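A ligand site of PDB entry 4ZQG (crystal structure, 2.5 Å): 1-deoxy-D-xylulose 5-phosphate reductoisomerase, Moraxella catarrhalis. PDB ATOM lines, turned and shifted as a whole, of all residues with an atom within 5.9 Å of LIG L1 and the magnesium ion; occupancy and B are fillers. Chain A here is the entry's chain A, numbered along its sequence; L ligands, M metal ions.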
ATOM      1  N   LYS A 129      10.514  17.345 -13.678  1.00  0.00           N
ATOM      2  CA  LYS A 129      11.775  16.628 -13.317  1.00  0.00           C
ATOM      3  C   LYS A 129      11.494  15.328 -12.550  1.00  0.00           C
ATOM      4  O   LYS A 129      12.255  14.363 -12.662  1.00  0.00           O
ATOM      5  CB  LYS A 129      12.714  17.518 -12.481  1.00  0.00           C
ATOM      6  CG  LYS A 129      12.099  17.922 -11.132  1.00  0.00           C
ATOM      7  CD  LYS A 129      12.950  18.937 -10.410  1.00  0.00           C
ATOM      8  CE  LYS A 129      13.122  20.195 -11.216  1.00  0.00           C
ATOM      9  NZ  LYS A 129      13.543  21.313 -10.328  1.00  0.00           N
ATOM     10  N   ILE A 153      13.988  22.130 -19.894  1.00  0.00           N
ATOM     11  CA  ILE A 153      13.420  23.430 -19.641  1.00  0.00           C
ATOM     12  C   ILE A 153      13.891  23.881 -18.303  1.00  0.00           C
ATOM     13  O   ILE A 153      13.983  25.071 -18.037  1.00  0.00           O
ATOM     14  CB  ILE A 153      11.866  23.328 -19.579  1.00  0.00           C
ATOM     15  CG1 ILE A 153      11.262  23.541 -20.956  1.00  0.00           C
ATOM     16  CG2 ILE A 153      11.212  24.290 -18.526  1.00  0.00           C
ATOM     17  CD1 ILE A 153       9.730  23.331 -20.950  1.00  0.00           C
ATOM     18  N   ASP A 154      14.110  22.931 -17.396  1.00  0.00           N
ATOM     19  CA  ASP A 154      14.659  23.254 -16.114  1.00  0.00           C
ATOM     20  C   ASP A 154      15.938  24.135 -16.309  1.00  0.00           C
ATOM     21  O   ASP A 154      16.785  23.845 -17.171  1.00  0.00           O
ATOM     22  CB  ASP A 154      14.951  21.973 -15.318  1.00  0.00           C
ATOM     23  CG  ASP A 154      14.982  22.244 -13.825  1.00  0.00           C
ATOM     24  OD1 ASP A 154      15.043  23.431 -13.508  1.00  0.00           O
ATOM     25  OD2 ASP A 154      14.910  21.314 -12.998  1.00  0.00           O
ATOM     26  N   SER A 155      16.047  25.204 -15.549  1.00  0.00           N
ATOM     27  CA  SER A 155      17.078  26.232 -15.748  1.00  0.00           C
ATOM     28  C   SER A 155      18.502  25.677 -15.792  1.00  0.00           C
ATOM     29  O   SER A 155      19.223  25.812 -16.796  1.00  0.00           O
ATOM     30  CB  SER A 155      16.998  27.284 -14.637  1.00  0.00           C
ATOM     31  OG  SER A 155      17.616  28.493 -15.031  1.00  0.00           O
ATOM     32  N   GLU A 156      18.858  24.982 -14.721  1.00  0.00           N
ATOM     33  CA  GLU A 156      20.171  24.381 -14.594  1.00  0.00           C
ATOM     34  C   GLU A 156      20.454  23.443 -15.748  1.00  0.00           C
ATOM     35  O   GLU A 156      21.516  23.507 -16.349  1.00  0.00           O
ATOM     36  CB  GLU A 156      20.319  23.669 -13.273  1.00  0.00           C
ATOM     37  CG  GLU A 156      20.079  24.571 -12.058  1.00  0.00           C
ATOM     38  CD  GLU A 156      18.612  24.785 -11.745  1.00  0.00           C
ATOM     39  OE1 GLU A 156      18.288  25.492 -10.764  1.00  0.00           O
ATOM     40  OE2 GLU A 156      17.802  24.219 -12.499  1.00  0.00           O
ATOM     41  N   HIS A 157      19.500  22.599 -16.104  1.00  0.00           N
ATOM     42  CA  HIS A 157      19.737  21.632 -17.157  1.00  0.00           C
ATOM     43  C   HIS A 157      19.754  22.302 -18.507  1.00  0.00           C
ATOM     44  O   HIS A 157      20.470  21.852 -19.414  1.00  0.00           O
ATOM     45  CB  HIS A 157      18.677  20.555 -17.107  1.00  0.00           C
ATOM     46  CG  HIS A 157      18.638  19.877 -15.787  1.00  0.00           C
ATOM     47  ND1 HIS A 157      18.091  20.476 -14.674  1.00  0.00           N
ATOM     48  CD2 HIS A 157      19.212  18.738 -15.355  1.00  0.00           C
ATOM     49  CE1 HIS A 157      18.269  19.700 -13.631  1.00  0.00           C
ATOM     50  NE2 HIS A 157      18.951  18.630 -14.011  1.00  0.00           N
ATOM     51  N   THR A 188      24.281  24.994 -10.028  1.00  0.00           N
ATOM     52  CA  THR A 188      24.149  26.141  -9.120  1.00  0.00           C
ATOM     53  C   THR A 188      22.848  25.995  -8.276  1.00  0.00           C
ATOM     54  O   THR A 188      21.872  25.478  -8.742  1.00  0.00           O
ATOM     55  CB  THR A 188      24.139  27.462  -9.928  1.00  0.00           C
ATOM     56  OG1 THR A 188      23.473  27.222 -11.192  1.00  0.00           O
ATOM     57  CG2 THR A 188      25.545  27.859 -10.239  1.00  0.00           C
ATOM     58  N   ALA A 189      22.875  26.462  -7.039  1.00  0.00           N
ATOM     59  CA  ALA A 189      21.750  26.397  -6.147  1.00  0.00           C
ATOM     60  C   ALA A 189      21.639  27.709  -5.404  1.00  0.00           C
ATOM     61  O   ALA A 189      22.652  28.212  -4.858  1.00  0.00           O
ATOM     62  CB  ALA A 189      22.003  25.302  -5.135  1.00  0.00           C
ATOM     63  N   SER A 190      20.420  28.277  -5.360  1.00  0.00           N
ATOM     64  CA  SER A 190      20.244  29.569  -4.687  1.00  0.00           C
ATOM     65  C   SER A 190      20.501  29.462  -3.203  1.00  0.00           C
ATOM     66  O   SER A 190      20.780  30.457  -2.541  1.00  0.00           O
ATOM     67  CB  SER A 190      18.861  30.120  -4.843  1.00  0.00           C
ATOM     68  OG  SER A 190      17.993  29.449  -3.954  1.00  0.00           O
ATOM     69  N   GLY A 191      20.362  28.262  -2.659  1.00  0.00           N
ATOM     70  CA  GLY A 191      20.424  28.088  -1.233  1.00  0.00           C
ATOM     71  C   GLY A 191      19.082  28.330  -0.580  1.00  0.00           C
ATOM     72  O   GLY A 191      18.955  28.112   0.616  1.00  0.00           O
ATOM     73  N   GLY A 192      18.107  28.810  -1.365  1.00  0.00           N
ATOM     74  CA  GLY A 192      16.734  29.103  -0.913  1.00  0.00           C
ATOM     75  C   GLY A 192      16.573  30.149   0.167  1.00  0.00           C
ATOM     76  O   GLY A 192      17.532  30.799   0.569  1.00  0.00           O
ATOM     77  N   HIS A 213      10.272  32.816  -2.441  1.00  0.00           N
ATOM     78  CA  HIS A 213      11.661  32.675  -2.807  1.00  0.00           C
ATOM     79  C   HIS A 213      12.176  34.044  -3.226  1.00  0.00           C
ATOM     80  O   HIS A 213      11.509  34.713  -3.995  1.00  0.00           O
ATOM     81  CB  HIS A 213      11.782  31.685  -3.969  1.00  0.00           C
ATOM     82  CG  HIS A 213      13.192  31.267  -4.287  1.00  0.00           C
ATOM     83  ND1 HIS A 213      14.126  32.140  -4.812  1.00  0.00           N
ATOM     84  CD2 HIS A 213      13.829  30.077  -4.173  1.00  0.00           C
ATOM     85  CE1 HIS A 213      15.273  31.510  -4.994  1.00  0.00           C
ATOM     86  NE2 HIS A 213      15.115  30.258  -4.608  1.00  0.00           N
ATOM     87  N   TRP A 216      12.844  33.792  -7.480  1.00  0.00           N
ATOM     88  CA  TRP A 216      12.012  33.042  -8.420  1.00  0.00           C
ATOM     89  C   TRP A 216      10.559  33.055  -7.950  1.00  0.00           C
ATOM     90  O   TRP A 216      10.316  33.042  -6.750  1.00  0.00           O
ATOM     91  CB  TRP A 216      12.448  31.580  -8.428  1.00  0.00           C
ATOM     92  CG  TRP A 216      13.694  31.254  -9.079  1.00  0.00           C
ATOM     93  CD1 TRP A 216      14.869  30.916  -8.468  1.00  0.00           C
ATOM     94  CD2 TRP A 216      13.915  31.144 -10.476  1.00  0.00           C
ATOM     95  NE1 TRP A 216      15.814  30.605  -9.420  1.00  0.00           N
ATOM     96  CE2 TRP A 216      15.256  30.743 -10.654  1.00  0.00           C
ATOM     97  CE3 TRP A 216      13.115  31.349 -11.613  1.00  0.00           C
ATOM     98  CZ2 TRP A 216      15.818  30.555 -11.899  1.00  0.00           C
ATOM     99  CZ3 TRP A 216      13.679  31.171 -12.848  1.00  0.00           C
ATOM    100  CH2 TRP A 216      15.018  30.761 -12.996  1.00  0.00           C
ATOM    101  N   MET A 218       7.385  30.504  -8.529  1.00  0.00           N
ATOM    102  CA  MET A 218       7.184  29.154  -9.031  1.00  0.00           C
ATOM    103  C   MET A 218       5.989  28.525  -8.374  1.00  0.00           C
ATOM    104  O   MET A 218       5.333  29.136  -7.521  1.00  0.00           O
ATOM    105  CB  MET A 218       8.423  28.316  -8.747  1.00  0.00           C
ATOM    106  CG  MET A 218       9.723  28.973  -9.165  1.00  0.00           C
ATOM    107  SD  MET A 218      11.136  28.043  -8.548  1.00  0.00           S
ATOM    108  CE  MET A 218      11.219  28.605  -6.844  1.00  0.00           C
ATOM    109  N   ILE A 222       8.103  22.831  -5.951  1.00  0.00           N
ATOM    110  CA  ILE A 222       9.433  23.261  -6.293  1.00  0.00           C
ATOM    111  C   ILE A 222       9.827  24.395  -5.354  1.00  0.00           C
ATOM    112  O   ILE A 222      10.934  24.462  -4.896  1.00  0.00           O
ATOM    113  CB  ILE A 222       9.578  23.619  -7.803  1.00  0.00           C
ATOM    114  CG1 ILE A 222      11.037  23.525  -8.220  1.00  0.00           C
ATOM    115  CG2 ILE A 222       9.088  25.000  -8.133  1.00  0.00           C
ATOM    116  CD1 ILE A 222      11.290  23.702  -9.706  1.00  0.00           C
ATOM    117  N   SER A 226      13.137  24.006  -2.911  1.00  0.00           N
ATOM    118  CA  SER A 226      14.251  24.931  -2.967  1.00  0.00           C
ATOM    119  C   SER A 226      14.663  25.343  -1.548  1.00  0.00           C
ATOM    120  O   SER A 226      15.830  25.344  -1.217  1.00  0.00           O
ATOM    121  CB  SER A 226      13.892  26.120  -3.841  1.00  0.00           C
ATOM    122  OG  SER A 226      14.881  27.093  -3.698  1.00  0.00           O
ATOM    123  N   ALA A 227      13.687  25.646  -0.706  1.00  0.00           N
ATOM    124  CA  ALA A 227      13.953  25.922   0.716  1.00  0.00           C
ATOM    125  C   ALA A 227      14.789  24.835   1.438  1.00  0.00           C
ATOM    126  O   ALA A 227      15.628  25.174   2.249  1.00  0.00           O
ATOM    127  CB  ALA A 227      12.629  26.153   1.450  1.00  0.00           C
ATOM    128  N   MET A 229      16.504  22.363  -0.182  1.00  0.00           N
ATOM    129  CA  MET A 229      17.538  21.987  -1.111  1.00  0.00           C
ATOM    130  C   MET A 229      17.351  20.600  -1.713  1.00  0.00           C
ATOM    131  O   MET A 229      18.183  20.123  -2.479  1.00  0.00           O
ATOM    132  CB  MET A 229      18.929  22.107  -0.504  1.00  0.00           C
ATOM    133  CG  MET A 229      20.020  22.153  -1.576  1.00  0.00           C
ATOM    134  SD  MET A 229      21.444  23.234  -1.306  1.00  0.00           S
ATOM    135  CE  MET A 229      20.563  24.719  -0.848  1.00  0.00           C
ATOM    136  N   ASN A 231      15.377  20.292  -4.065  1.00  0.00           N
ATOM    137  CA  ASN A 231      15.261  20.619  -5.495  1.00  0.00           C
ATOM    138  C   ASN A 231      16.586  20.337  -6.237  1.00  0.00           C
ATOM    139  O   ASN A 231      16.587  19.807  -7.363  1.00  0.00           O
ATOM    140  CB  ASN A 231      14.833  22.063  -5.696  1.00  0.00           C
ATOM    141  CG  ASN A 231      14.650  22.411  -7.177  1.00  0.00           C
ATOM    142  OD1 ASN A 231      13.914  21.750  -7.919  1.00  0.00           O
ATOM    143  ND2 ASN A 231      15.375  23.425  -7.626  1.00  0.00           N
ATOM    144  N   LYS A 232      17.706  20.650  -5.595  1.00  0.00           N
ATOM    145  CA  LYS A 232      18.998  20.358  -6.177  1.00  0.00           C
ATOM    146  C   LYS A 232      19.256  18.867  -6.205  1.00  0.00           C
ATOM    147  O   LYS A 232      19.787  18.346  -7.180  1.00  0.00           O
ATOM    148  CB  LYS A 232      20.101  21.084  -5.437  1.00  0.00           C
ATOM    149  CG  LYS A 232      21.156  21.659  -6.353  1.00  0.00           C
ATOM    150  CD  LYS A 232      20.596  22.346  -7.583  1.00  0.00           C
ATOM    151  CE  LYS A 232      19.627  23.458  -7.205  1.00  0.00           C
ATOM    152  NZ  LYS A 232      19.228  24.249  -8.398  1.00  0.00           N
ATOM    153  N   GLU A 235      17.400  17.568  -9.050  1.00  0.00           N
ATOM    154  CA  GLU A 235      18.066  18.064 -10.224  1.00  0.00           C
ATOM    155  C   GLU A 235      19.347  17.275 -10.491  1.00  0.00           C
ATOM    156  O   GLU A 235      19.677  16.989 -11.653  1.00  0.00           O
ATOM    157  CB  GLU A 235      18.315  19.558 -10.076  1.00  0.00           C
ATOM    158  CG  GLU A 235      17.043  20.320 -10.388  1.00  0.00           C
ATOM    159  CD  GLU A 235      17.166  21.788 -10.180  1.00  0.00           C
ATOM    160  OE1 GLU A 235      18.257  22.271  -9.793  1.00  0.00           O
ATOM    161  OE2 GLU A 235      16.165  22.431 -10.388  1.00  0.00           O
ATOM    162  N   SER A 258      21.335  33.799  -8.068  1.00  0.00           N
ATOM    163  CA  SER A 258      20.572  33.145  -9.150  1.00  0.00           C
ATOM    164  C   SER A 258      20.833  33.698 -10.566  1.00  0.00           C
ATOM    165  O   SER A 258      19.963  33.638 -11.455  1.00  0.00           O
ATOM    166  CB  SER A 258      19.073  33.071  -8.798  1.00  0.00           C
ATOM    167  OG  SER A 258      18.846  32.072  -7.819  1.00  0.00           O
ATOM    168  N   MET A 280      12.081  31.896 -16.160  1.00  0.00           N
ATOM    169  CA  MET A 280      11.996  30.679 -16.956  1.00  0.00           C
ATOM    170  C   MET A 280      11.655  30.882 -18.423  1.00  0.00           C
ATOM    171  O   MET A 280      11.691  29.939 -19.176  1.00  0.00           O
ATOM    172  CB  MET A 280      10.966  29.724 -16.359  1.00  0.00           C
ATOM    173  CG  MET A 280      11.361  29.141 -15.012  1.00  0.00           C
ATOM    174  SD  MET A 280      12.913  28.229 -15.006  1.00  0.00           S
ATOM    175  CE  MET A 280      12.596  26.892 -16.148  1.00  0.00           C
HETATM  176  O1  LIG L   1      14.652  25.021 -10.132  1.00  0.00           O
HETATM  177  N1  LIG L   1      14.655  26.374 -10.441  1.00  0.00           N
HETATM  178  C1  LIG L   1      14.868  26.780 -11.622  1.00  0.00           C
HETATM  179  O2  LIG L   1      15.097  26.001 -12.531  1.00  0.00           O
HETATM  180  C2  LIG L   1      14.463  27.255  -9.295  1.00  0.00           C
HETATM  181  C3  LIG L   1      15.710  26.868  -8.483  1.00  0.00           C
HETATM  182  C4  LIG L   1      15.690  27.470  -7.110  1.00  0.00           C
HETATM  183  P1  LIG L   1      17.128  26.795  -6.300  1.00  0.00           P
HETATM  184  O3  LIG L   1      18.402  27.354  -7.086  1.00  0.00           O
HETATM  185  O4  LIG L   1      17.183  25.354  -6.539  1.00  0.00           O
HETATM  186  O5  LIG L   1      17.236  27.105  -4.708  1.00  0.00           O
HETATM  187  P1  LG2 L   2       2.461  24.249 -10.735  1.00  0.00           P
HETATM  188  O1  LG2 L   2       2.120  23.636  -9.417  1.00  0.00           O
HETATM  189  O2  LG2 L   2       2.501  25.752 -10.908  1.00  0.00           O
HETATM  190  O3  LG2 L   2       1.590  23.611 -11.938  1.00  0.00           O
HETATM  191  C1  LG2 L   2       1.462  22.224 -12.168  1.00  0.00           C
HETATM  192  C2  LG2 L   2       0.586  21.952 -13.412  1.00  0.00           C
HETATM  193  O4  LG2 L   2       0.348  20.529 -13.451  1.00  0.00           O
HETATM  194  C3  LG2 L   2      -0.770  22.656 -13.382  1.00  0.00           C
HETATM  195  O5  LG2 L   2      -1.184  23.081 -14.685  1.00  0.00           O
HETATM  196  C4  LG2 L   2      -1.712  21.571 -12.861  1.00  0.00           C
HETATM  197  O6  LG2 L   2      -3.012  21.618 -13.443  1.00  0.00           O
HETATM  198  C5  LG2 L   2      -1.044  20.259 -13.244  1.00  0.00           C
HETATM  199  N1  LG2 L   2      -1.260  19.210 -12.204  1.00  0.00           N
HETATM  200  C6  LG2 L   2      -1.047  19.361 -10.878  1.00  0.00           C
HETATM  201  N2  LG2 L   2      -1.348  18.225 -10.205  1.00  0.00           N
HETATM  202  C7  LG2 L   2      -1.771  17.321 -11.090  1.00  0.00           C
HETATM  203  C8  LG2 L   2      -2.249  15.926 -10.981  1.00  0.00           C
HETATM  204  N3  LG2 L   2      -2.308  15.300  -9.763  1.00  0.00           N
HETATM  205  N4  LG2 L   2      -2.601  15.347 -12.145  1.00  0.00           N
HETATM  206  C9  LG2 L   2      -2.558  15.997 -13.344  1.00  0.00           C
HETATM  207  N5  LG2 L   2      -2.144  17.269 -13.520  1.00  0.00           N
HETATM  208  C10 LG2 L   2      -1.728  17.967 -12.419  1.00  0.00           C
HETATM  209  O7  LG2 L   2       3.896  23.631 -11.137  1.00  0.00           O
HETATM  210  P2  LG2 L   2       5.209  24.352 -11.717  1.00  0.00           P
HETATM  211  O8  LG2 L   2       5.806  25.101 -10.538  1.00  0.00           O
HETATM  212  O9  LG2 L   2       4.851  24.970 -13.045  1.00  0.00           O
HETATM  213  O10 LG2 L   2       6.067  23.020 -11.979  1.00  0.00           O
HETATM  214  C11 LG2 L   2       5.889  22.226 -13.147  1.00  0.00           C
HETATM  215  C12 LG2 L   2       7.065  21.256 -13.309  1.00  0.00           C
HETATM  216  O11 LG2 L   2       8.214  21.916 -13.858  1.00  0.00           O
HETATM  217  C13 LG2 L   2       7.482  20.679 -11.972  1.00  0.00           C
HETATM  218  O12 LG2 L   2       7.890  19.338 -12.194  1.00  0.00           O
HETATM  219  C14 LG2 L   2       8.615  21.564 -11.517  1.00  0.00           C
HETATM  220  O13 LG2 L   2       9.473  20.885 -10.587  1.00  0.00           O
HETATM  221  C15 LG2 L   2       9.258  21.928 -12.858  1.00  0.00           C
HETATM  222  N6  LG2 L   2       9.933  23.240 -12.824  1.00  0.00           N
HETATM  223  C16 LG2 L   2       9.234  24.380 -12.577  1.00  0.00           C
HETATM  224  C17 LG2 L   2       9.886  25.626 -12.512  1.00  0.00           C
HETATM  225  C18 LG2 L   2       9.153  26.915 -12.259  1.00  0.00           C
HETATM  226  O14 LG2 L   2       9.693  27.980 -12.499  1.00  0.00           O
HETATM  227  N7  LG2 L   2       7.898  26.902 -11.799  1.00  0.00           N
HETATM  228  C19 LG2 L   2      11.258  25.676 -12.713  1.00  0.00           C
HETATM  229  C20 LG2 L   2      11.921  24.501 -12.980  1.00  0.00           C
HETATM  230  C21 LG2 L   2      11.254  23.289 -13.035  1.00  0.00           C
HETATM  231 MG    MG M   1      15.819  24.125 -11.677  1.00  0.00          MG
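NE2 of His 157 is in hydrogen-bond range of O of Glu 235 (3.0 Å).
The side-chain amino group (NZ) of Lys 129 is in salt-bridge range of the side-chain carboxylate (OD2) of Asp 154 (3.0 Å).
OE2 of Glu 235 lies close to ND2 of Asn 231, at 3.0 Å.
The side-chain amino group of Lys 232 is in salt-bridge range of the side-chain carboxylate of Glu 156 (2.8 Å).
OG of Ser 190 is in hydrogen-bond range of NE2 of His 213, 3.1 Å away.
NZ of Lys 129 is in hydrogen-bond range of OD1 of Asn 231 (2.5 Å).
The side-chain amino group (NZ) of Lys 232 lies within salt-bridge range of the side-chain carboxylate (OE1) of Glu 235, 2.6 Å away.
The side-chain hydroxyl (OG) of Ser 226 sits close to a ring nitrogen (NE2) of His 213, 3.3 Å away.
Lys 129 touches the magnesium ion (NZ to MG, 3.9 Å).
The nearest printed residue that does not touch the magnesium ion is Ser 155 (4.03 Å).
Merely in contact with LIG L1: Lys 129 (3.9 Å), Ala 189 (3.6 Å), Gly 191 (3.9 Å), Gly 192 (3.9 Å), His 213 (3.8 Å), Trp 216 (3.6 Å), Met 218 (3.5 Å), Ile 222 (3.6 Å) and Met 280 (3.98 Å).
Of the 23 residues printed, 17 come within 4 Å of LIG L1.
The magnesium ion is bound by OD1 of Asp 154, O1 of LIG L1, OE2 of Glu 156, OE2 of Glu 235 and O2 of LIG L1.
OG of Ser 190 lies within hydrogen-bond range of O5 of LIG L1 (2.6 Å).
OG of Ser 226 lies within hydrogen-bond range of O5 of LIG L1.
N of Ser 190 is in hydrogen-bond range of O3 of LIG L1, at 2.8 Å.
The backbone NH (N) of Ser 155 lies close to an oxygen (O2) of LIG L1 (3.3 Å).
ND2 of Asn 231 is in hydrogen-bond range of O4 of LIG L1 (2.9 Å).
NZ of Lys 232 lies within salt-bridge range of O4 of LIG L1 (3.0 Å).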
